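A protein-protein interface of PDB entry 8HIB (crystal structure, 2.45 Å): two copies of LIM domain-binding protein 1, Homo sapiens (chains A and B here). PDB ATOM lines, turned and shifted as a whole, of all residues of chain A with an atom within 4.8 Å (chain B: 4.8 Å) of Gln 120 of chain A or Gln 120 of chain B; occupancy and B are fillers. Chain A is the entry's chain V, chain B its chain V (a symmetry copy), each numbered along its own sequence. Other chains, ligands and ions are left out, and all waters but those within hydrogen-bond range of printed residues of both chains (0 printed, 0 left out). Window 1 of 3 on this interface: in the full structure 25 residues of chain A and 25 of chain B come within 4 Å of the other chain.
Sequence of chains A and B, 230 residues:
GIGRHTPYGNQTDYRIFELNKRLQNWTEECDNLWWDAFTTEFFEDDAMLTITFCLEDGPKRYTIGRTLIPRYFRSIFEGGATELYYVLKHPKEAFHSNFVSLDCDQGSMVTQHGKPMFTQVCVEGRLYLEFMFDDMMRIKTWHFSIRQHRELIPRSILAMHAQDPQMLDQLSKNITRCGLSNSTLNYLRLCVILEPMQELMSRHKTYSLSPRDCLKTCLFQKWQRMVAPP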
ATOM      1  N   TYR A  85     -18.179 -21.552  16.571  1.00  0.00           N
ATOM      2  CA  TYR A  85     -19.177 -22.228  17.402  1.00  0.00           C
ATOM      3  C   TYR A  85     -20.312 -22.735  16.543  1.00  0.00           C
ATOM      4  O   TYR A  85     -20.504 -22.310  15.408  1.00  0.00           O
ATOM      5  CB  TYR A  85     -19.717 -21.329  18.528  1.00  0.00           C
ATOM      6  CG  TYR A  85     -20.401 -20.042  18.116  1.00  0.00           C
ATOM      7  CD1 TYR A  85     -19.677 -18.871  17.952  1.00  0.00           C
ATOM      8  CD2 TYR A  85     -21.788 -19.977  17.964  1.00  0.00           C
ATOM      9  CE1 TYR A  85     -20.317 -17.655  17.637  1.00  0.00           C
ATOM     10  CE2 TYR A  85     -22.442 -18.777  17.644  1.00  0.00           C
ATOM     11  CZ  TYR A  85     -21.708 -17.637  17.470  1.00  0.00           C
ATOM     12  OH  TYR A  85     -22.351 -16.482  17.128  1.00  0.00           O
ATOM     13  N   VAL A 110     -20.662 -21.125  12.862  1.00  0.00           N
ATOM     14  CA  VAL A 110     -20.411 -19.689  12.904  1.00  0.00           C
ATOM     15  C   VAL A 110     -18.917 -19.452  13.147  1.00  0.00           C
ATOM     16  O   VAL A 110     -18.310 -20.073  14.030  1.00  0.00           O
ATOM     17  CB  VAL A 110     -21.288 -19.005  13.974  1.00  0.00           C
ATOM     18  CG1 VAL A 110     -21.060 -17.511  14.017  1.00  0.00           C
ATOM     19  CG2 VAL A 110     -22.797 -19.282  13.718  1.00  0.00           C
ATOM     20  N   THR A 111     -18.312 -18.608  12.325  1.00  0.00           N
ATOM     21  CA  THR A 111     -16.911 -18.244  12.501  1.00  0.00           C
ATOM     22  C   THR A 111     -16.751 -16.733  12.379  1.00  0.00           C
ATOM     23  O   THR A 111     -17.429 -16.073  11.585  1.00  0.00           O
ATOM     24  CB  THR A 111     -15.975 -18.952  11.489  1.00  0.00           C
ATOM     25  OG1 THR A 111     -16.516 -18.825  10.174  1.00  0.00           O
ATOM     26  CG2 THR A 111     -15.833 -20.431  11.836  1.00  0.00           C
ATOM     27  N   GLN A 112     -15.864 -16.188  13.192  1.00  0.00           N
ATOM     28  CA  GLN A 112     -15.564 -14.767  13.199  1.00  0.00           C
ATOM     29  C   GLN A 112     -14.135 -14.619  12.691  1.00  0.00           C
ATOM     30  O   GLN A 112     -13.231 -15.277  13.209  1.00  0.00           O
ATOM     31  CB  GLN A 112     -15.738 -14.206  14.617  1.00  0.00           C
ATOM     32  CG  GLN A 112     -15.569 -12.710  14.797  1.00  0.00           C
ATOM     33  CD  GLN A 112     -16.422 -11.906  13.852  1.00  0.00           C
ATOM     34  OE1 GLN A 112     -17.641 -12.147  13.734  1.00  0.00           O
ATOM     35  NE2 GLN A 112     -15.785 -10.961  13.127  1.00  0.00           N
ATOM     36  N   PHE A 118     -13.067  -7.536   9.462  1.00  0.00           N
ATOM     37  CA  PHE A 118     -13.538  -8.648  10.279  1.00  0.00           C
ATOM     38  C   PHE A 118     -14.802  -9.125   9.590  1.00  0.00           C
ATOM     39  O   PHE A 118     -15.723  -8.336   9.423  1.00  0.00           O
ATOM     40  CB  PHE A 118     -13.751  -8.195  11.729  1.00  0.00           C
ATOM     41  CG  PHE A 118     -12.548  -7.558  12.353  1.00  0.00           C
ATOM     42  CD1 PHE A 118     -12.114  -6.294  11.953  1.00  0.00           C
ATOM     43  CD2 PHE A 118     -11.860  -8.204  13.364  1.00  0.00           C
ATOM     44  CE1 PHE A 118     -11.002  -5.702  12.528  1.00  0.00           C
ATOM     45  CE2 PHE A 118     -10.750  -7.616  13.951  1.00  0.00           C
ATOM     46  CZ  PHE A 118     -10.319  -6.356  13.530  1.00  0.00           C
ATOM     47  N   THR A 119     -14.880 -10.383   9.180  1.00  0.00           N
ATOM     48  CA  THR A 119     -16.058 -10.851   8.472  1.00  0.00           C
ATOM     49  C   THR A 119     -16.558 -12.052   9.268  1.00  0.00           C
ATOM     50  O   THR A 119     -15.777 -12.791   9.885  1.00  0.00           O
ATOM     51  CB  THR A 119     -15.867 -11.220   6.991  1.00  0.00           C
ATOM     52  OG1 THR A 119     -16.951 -12.050   6.564  1.00  0.00           O
ATOM     53  CG2 THR A 119     -14.616 -11.977   6.783  1.00  0.00           C
ATOM     54  N   GLN A 120     -17.871 -12.240   9.275  1.00  0.00           N
ATOM     55  CA  GLN A 120     -18.467 -13.378   9.962  1.00  0.00           C
ATOM     56  C   GLN A 120     -19.090 -14.305   8.934  1.00  0.00           C
ATOM     57  O   GLN A 120     -19.808 -13.854   8.038  1.00  0.00           O
ATOM     58  CB  GLN A 120     -19.514 -12.941  10.985  1.00  0.00           C
ATOM     59  CG  GLN A 120     -20.393 -14.093  11.488  1.00  0.00           C
ATOM     60  CD  GLN A 120     -21.086 -13.730  12.786  1.00  0.00           C
ATOM     61  OE1 GLN A 120     -20.503 -13.045  13.625  1.00  0.00           O
ATOM     62  NE2 GLN A 120     -22.323 -14.184  12.965  1.00  0.00           N
ATOM     63  N   VAL A 121     -18.810 -15.586   9.063  1.00  0.00           N
ATOM     64  CA  VAL A 121     -19.310 -16.600   8.151  1.00  0.00           C
ATOM     65  C   VAL A 121     -20.272 -17.489   8.926  1.00  0.00           C
ATOM     66  O   VAL A 121     -19.949 -17.975  10.024  1.00  0.00           O
ATOM     67  CB  VAL A 121     -18.153 -17.408   7.529  1.00  0.00           C
ATOM     68  CG1 VAL A 121     -18.692 -18.534   6.692  1.00  0.00           C
ATOM     69  CG2 VAL A 121     -17.274 -16.493   6.663  1.00  0.00           C
ATOM     70  N   CYS A 122     -21.466 -17.670   8.372  1.00  0.00           N
ATOM     71  CA  CYS A 122     -22.502 -18.505   8.954  1.00  0.00           C
ATOM     72  C   CYS A 122     -22.862 -19.579   7.944  1.00  0.00           C
ATOM     73  O   CYS A 122     -23.367 -19.275   6.857  1.00  0.00           O
ATOM     74  CB  CYS A 122     -23.729 -17.680   9.322  1.00  0.00           C
ATOM     75  SG  CYS A 122     -24.977 -18.729  10.119  1.00  0.00           S
ATOM     76  N   ARG A 150     -23.740 -17.742   4.526  1.00  0.00           N
ATOM     77  CA  ARG A 150     -23.857 -16.298   4.407  1.00  0.00           C
ATOM     78  C   ARG A 150     -22.580 -15.713   4.961  1.00  0.00           C
ATOM     79  O   ARG A 150     -21.898 -16.345   5.767  1.00  0.00           O
ATOM     80  CB  ARG A 150     -25.027 -15.693   5.200  1.00  0.00           C
ATOM     81  CG  ARG A 150     -26.363 -15.553   4.501  1.00  0.00           C
ATOM     82  CD  ARG A 150     -27.400 -16.313   5.345  1.00  0.00           C
ATOM     83  NE  ARG A 150     -27.290 -15.965   6.760  1.00  0.00           N
ATOM     84  CZ  ARG A 150     -27.393 -16.841   7.755  1.00  0.00           C
ATOM     85  NH1 ARG A 150     -27.416 -18.155   7.524  1.00  0.00           N
ATOM     86  NH2 ARG A 150     -27.415 -16.392   9.014  1.00  0.00           N
ATOM     87  N   GLU A 151     -22.283 -14.486   4.551  1.00  0.00           N
ATOM     88  CA  GLU A 151     -21.083 -13.786   4.979  1.00  0.00           C
ATOM     89  C   GLU A 151     -21.495 -12.379   5.374  1.00  0.00           C
ATOM     90  O   GLU A 151     -22.147 -11.682   4.591  1.00  0.00           O
ATOM     91  CB  GLU A 151     -20.027 -13.775   3.866  1.00  0.00           C
ATOM     92  CG  GLU A 151     -19.619 -15.187   3.410  1.00  0.00           C
ATOM     93  CD  GLU A 151     -18.383 -15.226   2.511  1.00  0.00           C
ATOM     94  OE1 GLU A 151     -17.642 -14.226   2.441  1.00  0.00           O
ATOM     95  OE2 GLU A 151     -18.118 -16.291   1.917  1.00  0.00           O
ATOM     96  N   LEU A 152     -21.142 -11.965   6.587  1.00  0.00           N
ATOM     97  CA  LEU A 152     -21.652 -10.722   7.145  1.00  0.00           C
ATOM     98  C   LEU A 152     -20.527  -9.714   7.313  1.00  0.00           C
ATOM     99  O   LEU A 152     -19.409 -10.070   7.699  1.00  0.00           O
ATOM    100  CB  LEU A 152     -22.335 -10.960   8.487  1.00  0.00           C
ATOM    101  CG  LEU A 152     -23.366 -12.088   8.522  1.00  0.00           C
ATOM    102  CD1 LEU A 152     -23.851 -12.252   9.948  1.00  0.00           C
ATOM    103  CD2 LEU A 152     -24.517 -11.751   7.588  1.00  0.00           C
ATOM    104  N   TYR B  85     -29.720 -14.676  21.246  1.00  0.00           N
ATOM    105  CA  TYR B  85     -28.959 -15.564  22.129  1.00  0.00           C
ATOM    106  C   TYR B  85     -27.788 -14.821  22.729  1.00  0.00           C
ATOM    107  O   TYR B  85     -27.372 -13.771  22.248  1.00  0.00           O
ATOM    108  CB  TYR B  85     -28.476 -16.837  21.414  1.00  0.00           C
ATOM    109  CG  TYR B  85     -27.569 -16.653  20.214  1.00  0.00           C
ATOM    110  CD1 TYR B  85     -28.093 -16.511  18.939  1.00  0.00           C
ATOM    111  CD2 TYR B  85     -26.178 -16.700  20.346  1.00  0.00           C
ATOM    112  CE1 TYR B  85     -27.253 -16.411  17.811  1.00  0.00           C
ATOM    113  CE2 TYR B  85     -25.326 -16.595  19.236  1.00  0.00           C
ATOM    114  CZ  TYR B  85     -25.864 -16.439  17.988  1.00  0.00           C
ATOM    115  OH  TYR B  85     -25.026 -16.305  16.919  1.00  0.00           O
ATOM    116  N   VAL B 110     -26.675 -11.403  20.901  1.00  0.00           N
ATOM    117  CA  VAL B 110     -26.731 -11.554  19.452  1.00  0.00           C
ATOM    118  C   VAL B 110     -28.198 -11.614  19.014  1.00  0.00           C
ATOM    119  O   VAL B 110     -29.009 -12.339  19.605  1.00  0.00           O
ATOM    120  CB  VAL B 110     -25.939 -12.798  18.994  1.00  0.00           C
ATOM    121  CG1 VAL B 110     -25.965 -12.959  17.491  1.00  0.00           C
ATOM    122  CG2 VAL B 110     -24.461 -12.723  19.472  1.00  0.00           C
ATOM    123  N   THR B 111     -28.552 -10.806  18.026  1.00  0.00           N
ATOM    124  CA  THR B 111     -29.900 -10.825  17.471  1.00  0.00           C
ATOM    125  C   THR B 111     -29.833 -10.836  15.949  1.00  0.00           C
ATOM    126  O   THR B 111     -28.960 -10.212  15.337  1.00  0.00           O
ATOM    127  CB  THR B 111     -30.762  -9.629  17.948  1.00  0.00           C
ATOM    128  OG1 THR B 111     -30.019  -8.419  17.799  1.00  0.00           O
ATOM    129  CG2 THR B 111     -31.156  -9.802  19.412  1.00  0.00           C
ATOM    130  N   GLN B 112     -30.748 -11.570  15.344  1.00  0.00           N
ATOM    131  CA  GLN B 112     -30.850 -11.679  13.899  1.00  0.00           C
ATOM    132  C   GLN B 112     -32.152 -10.998  13.498  1.00  0.00           C
ATOM    133  O   GLN B 112     -33.205 -11.318  14.053  1.00  0.00           O
ATOM    134  CB  GLN B 112     -30.815 -13.157  13.486  1.00  0.00           C
ATOM    135  CG  GLN B 112     -30.803 -13.462  12.000  1.00  0.00           C
ATOM    136  CD  GLN B 112     -29.716 -12.727  11.260  1.00  0.00           C
ATOM    137  OE1 GLN B 112     -28.538 -12.753  11.670  1.00  0.00           O
ATOM    138  NE2 GLN B 112     -30.103 -12.021  10.176  1.00  0.00           N
ATOM    139  N   PHE B 118     -31.748  -8.384   6.100  1.00  0.00           N
ATOM    140  CA  PHE B 118     -31.561  -9.141   7.332  1.00  0.00           C
ATOM    141  C   PHE B 118     -30.285  -8.586   7.936  1.00  0.00           C
ATOM    142  O   PHE B 118     -29.250  -8.628   7.283  1.00  0.00           O
ATOM    143  CB  PHE B 118     -31.507 -10.645   7.033  1.00  0.00           C
ATOM    144  CG  PHE B 118     -32.692 -11.160   6.276  1.00  0.00           C
ATOM    145  CD1 PHE B 118     -32.885 -10.834   4.933  1.00  0.00           C
ATOM    146  CD2 PHE B 118     -33.605 -11.997   6.890  1.00  0.00           C
ATOM    147  CE1 PHE B 118     -33.978 -11.308   4.229  1.00  0.00           C
ATOM    148  CE2 PHE B 118     -34.700 -12.484   6.192  1.00  0.00           C
ATOM    149  CZ  PHE B 118     -34.887 -12.136   4.852  1.00  0.00           C
ATOM    150  N   THR B 119     -30.320  -8.066   9.154  1.00  0.00           N
ATOM    151  CA  THR B 119     -29.124  -7.483   9.736  1.00  0.00           C
ATOM    152  C   THR B 119     -28.918  -8.214  11.057  1.00  0.00           C
ATOM    153  O   THR B 119     -29.875  -8.642  11.718  1.00  0.00           O
ATOM    154  CB  THR B 119     -29.140  -5.960   9.953  1.00  0.00           C
ATOM    155  OG1 THR B 119     -28.128  -5.604  10.898  1.00  0.00           O
ATOM    156  CG2 THR B 119     -30.437  -5.507  10.494  1.00  0.00           C
ATOM    157  N   GLN B 120     -27.658  -8.382  11.440  1.00  0.00           N
ATOM    158  CA  GLN B 120     -27.333  -9.025  12.705  1.00  0.00           C
ATOM    159  C   GLN B 120     -26.696  -8.003  13.630  1.00  0.00           C
ATOM    160  O   GLN B 120     -25.796  -7.264  13.222  1.00  0.00           O
ATOM    161  CB  GLN B 120     -26.401 -10.221  12.513  1.00  0.00           C
ATOM    162  CG  GLN B 120     -25.773 -10.720  13.820  1.00  0.00           C
ATOM    163  CD  GLN B 120     -25.239 -12.131  13.670  1.00  0.00           C
ATOM    164  OE1 GLN B 120     -25.841 -12.947  12.975  1.00  0.00           O
ATOM    165  NE2 GLN B 120     -24.115 -12.430  14.317  1.00  0.00           N
ATOM    166  N   VAL B 121     -27.163  -7.965  14.861  1.00  0.00           N
ATOM    167  CA  VAL B 121     -26.676  -7.032  15.863  1.00  0.00           C
ATOM    168  C   VAL B 121     -25.972  -7.837  16.945  1.00  0.00           C
ATOM    169  O   VAL B 121     -26.518  -8.827  17.463  1.00  0.00           O
ATOM    170  CB  VAL B 121     -27.826  -6.179  16.435  1.00  0.00           C
ATOM    171  CG1 VAL B 121     -27.327  -5.313  17.559  1.00  0.00           C
ATOM    172  CG2 VAL B 121     -28.432  -5.298  15.333  1.00  0.00           C
ATOM    173  N   CYS B 122     -24.744  -7.436  17.257  1.00  0.00           N
ATOM    174  CA  CYS B 122     -23.931  -8.066  18.281  1.00  0.00           C
ATOM    175  C   CYS B 122     -23.573  -7.012  19.313  1.00  0.00           C
ATOM    176  O   CYS B 122     -22.875  -6.041  19.002  1.00  0.00           O
ATOM    177  CB  CYS B 122     -22.671  -8.681  17.681  1.00  0.00           C
ATOM    178  SG  CYS B 122     -21.712  -9.530  18.965  1.00  0.00           S
ATOM    179  N   ARG B 150     -21.951  -3.949  17.361  1.00  0.00           N
ATOM    180  CA  ARG B 150     -21.622  -3.993  15.945  1.00  0.00           C
ATOM    181  C   ARG B 150     -22.876  -4.423  15.222  1.00  0.00           C
ATOM    182  O   ARG B 150     -23.750  -5.061  15.809  1.00  0.00           O
ATOM    183  CB  ARG B 150     -20.512  -4.995  15.588  1.00  0.00           C
ATOM    184  CG  ARG B 150     -19.080  -4.502  15.593  1.00  0.00           C
ATOM    185  CD  ARG B 150     -18.294  -5.399  16.565  1.00  0.00           C
ATOM    186  NE  ARG B 150     -18.566  -6.814  16.319  1.00  0.00           N
ATOM    187  CZ  ARG B 150     -18.735  -7.720  17.278  1.00  0.00           C
ATOM    188  NH1 ARG B 150     -18.856  -7.364  18.558  1.00  0.00           N
ATOM    189  NH2 ARG B 150     -18.840  -9.010  16.939  1.00  0.00           N
ATOM    190  N   GLU B 151     -22.937  -4.103  13.936  1.00  0.00           N
ATOM    191  CA  GLU B 151     -24.081  -4.431  13.100  1.00  0.00           C
ATOM    192  C   GLU B 151     -23.544  -5.018  11.807  1.00  0.00           C
ATOM    193  O   GLU B 151     -22.693  -4.405  11.155  1.00  0.00           O
ATOM    194  CB  GLU B 151     -24.947  -3.191  12.843  1.00  0.00           C
ATOM    195  CG  GLU B 151     -25.471  -2.543  14.137  1.00  0.00           C
ATOM    196  CD  GLU B 151     -26.552  -1.485  13.918  1.00  0.00           C
ATOM    197  OE1 GLU B 151     -27.131  -1.415  12.816  1.00  0.00           O
ATOM    198  OE2 GLU B 151     -26.868  -0.757  14.881  1.00  0.00           O
ATOM    199  N   LEU B 152     -24.015  -6.207  11.444  1.00  0.00           N
ATOM    200  CA  LEU B 152     -23.429  -6.952  10.339  1.00  0.00           C
ATOM    201  C   LEU B 152     -24.419  -7.064   9.191  1.00  0.00           C
ATOM    202  O   LEU B 152     -25.620  -7.256   9.406  1.00  0.00           O
ATOM    203  CB  LEU B 152     -22.993  -8.343  10.784  1.00  0.00           C
ATOM    204  CG  LEU B 152     -22.143  -8.405  12.053  1.00  0.00           C
ATOM    205  CD1 LEU B 152     -21.904  -9.860  12.401  1.00  0.00           C
ATOM    206  CD2 LEU B 152     -20.830  -7.675  11.818  1.00  0.00           C
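The backbone carbonyl oxygen (O) of Gln 120 of chain B is in hydrogen-bond range of the backbone NH (N) of Leu 152 of chain B (2.7 Å). The backbone NH of Val 110 of chain B sits at hydrogen-bond distance from the backbone carbonyl oxygen of Tyr 85 of chain B, at 2.8 Å. The side-chain amide oxygen (OE1) of Gln 112 of chain B lies close to the side-chain amide oxygen (OE1) of Gln 120 of chain B (3.0 Å). The side-chain hydroxyl (OG1) of Thr 119 of chain B is in hydrogen-bond range of the backbone carbonyl oxygen (O) of Leu 152 of chain B, 3.4 Å away. The side-chain amide oxygen (OE1) of Gln 120 of chain A sits close to the side-chain amide oxygen (OE1) of Gln 112 of chain A, at 3.0 Å. The backbone carbonyl oxygen of Tyr 85 of chain A is in hydrogen-bond range of the backbone NH of Val 110 of chain A (2.8 Å).
OH of Tyr 85 of chain A lies within hydrogen-bond range of OH of Tyr 85 of chain B (2.7 Å). The side-chain amide nitrogen (NE2) of Gln 120 of chain A lies close to the side-chain amide nitrogen (NE2) of Gln 120 of chain B (2.8 Å).
Of the 12 printed residues of chain A, 3 touch a printed residue of chain B. Printed residues of chain A that touch a printed residue of chain B: Tyr 85, Gln 120 and Leu 152. Printed residues of chain B that touch a printed residue of chain A: Tyr 85, Gln 120 and Leu 152. Hydrophobic or aromatic side chains of chain B that line the printed part of chain A: Tyr 85 and Leu 152. Among the printed residues, 5 pairs touch across the chains. Among the printed residues, no Asp or Glu carboxylate lies within 4 Å of a Lys or Arg side-chain nitrogen of the other chain.
Among the printed residues, merely in contact across the chains: Gln 120 of chain A with Leu 152 of chain B, Leu 152 of chain A with Gln 120 of chain B and Leu 152 of chain A with Leu 152 of chain B.
Gln 120 of chain A touches two residues of chain B. Printed residues of chain A within 4 Å of Tyr 85 of chain B: Tyr 85. Phe 118 of chain B touches none of the printed residues of chain A. Of chain A, only Gln 120 and Leu 152 come within 4 Å of Gln 120 of chain B. Of the printed residues of chain A, Leu 152 of chain B touches Gln 120 (3.7 Å) and Leu 152 (3.5 Å). The nearest printed residue of chain B that does not touch Tyr 85 of chain A is Val 110 of chain B (4.9 Å).
Tyr 85 of chain A touches its own counterpart, Tyr 85 of chain B. Gln 120 of chain B touches its own counterpart, Gln 120 of chain A. Gln 120 of chain A touches Leu 152 of chain B, and with the chains exchanged Leu 152 of chain A touches Gln 120 of chain B. Leu 152 of chain B touches its own counterpart, Leu 152 of chain A. Positions printed for both chains: 85, 110, 111, 112, 118, 119, 120, 121, 122, 150, 151 and 152. Of the 5 pairs that touch across the chains among the printed residues, 5 have their exchanged pair printed and touching as well.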
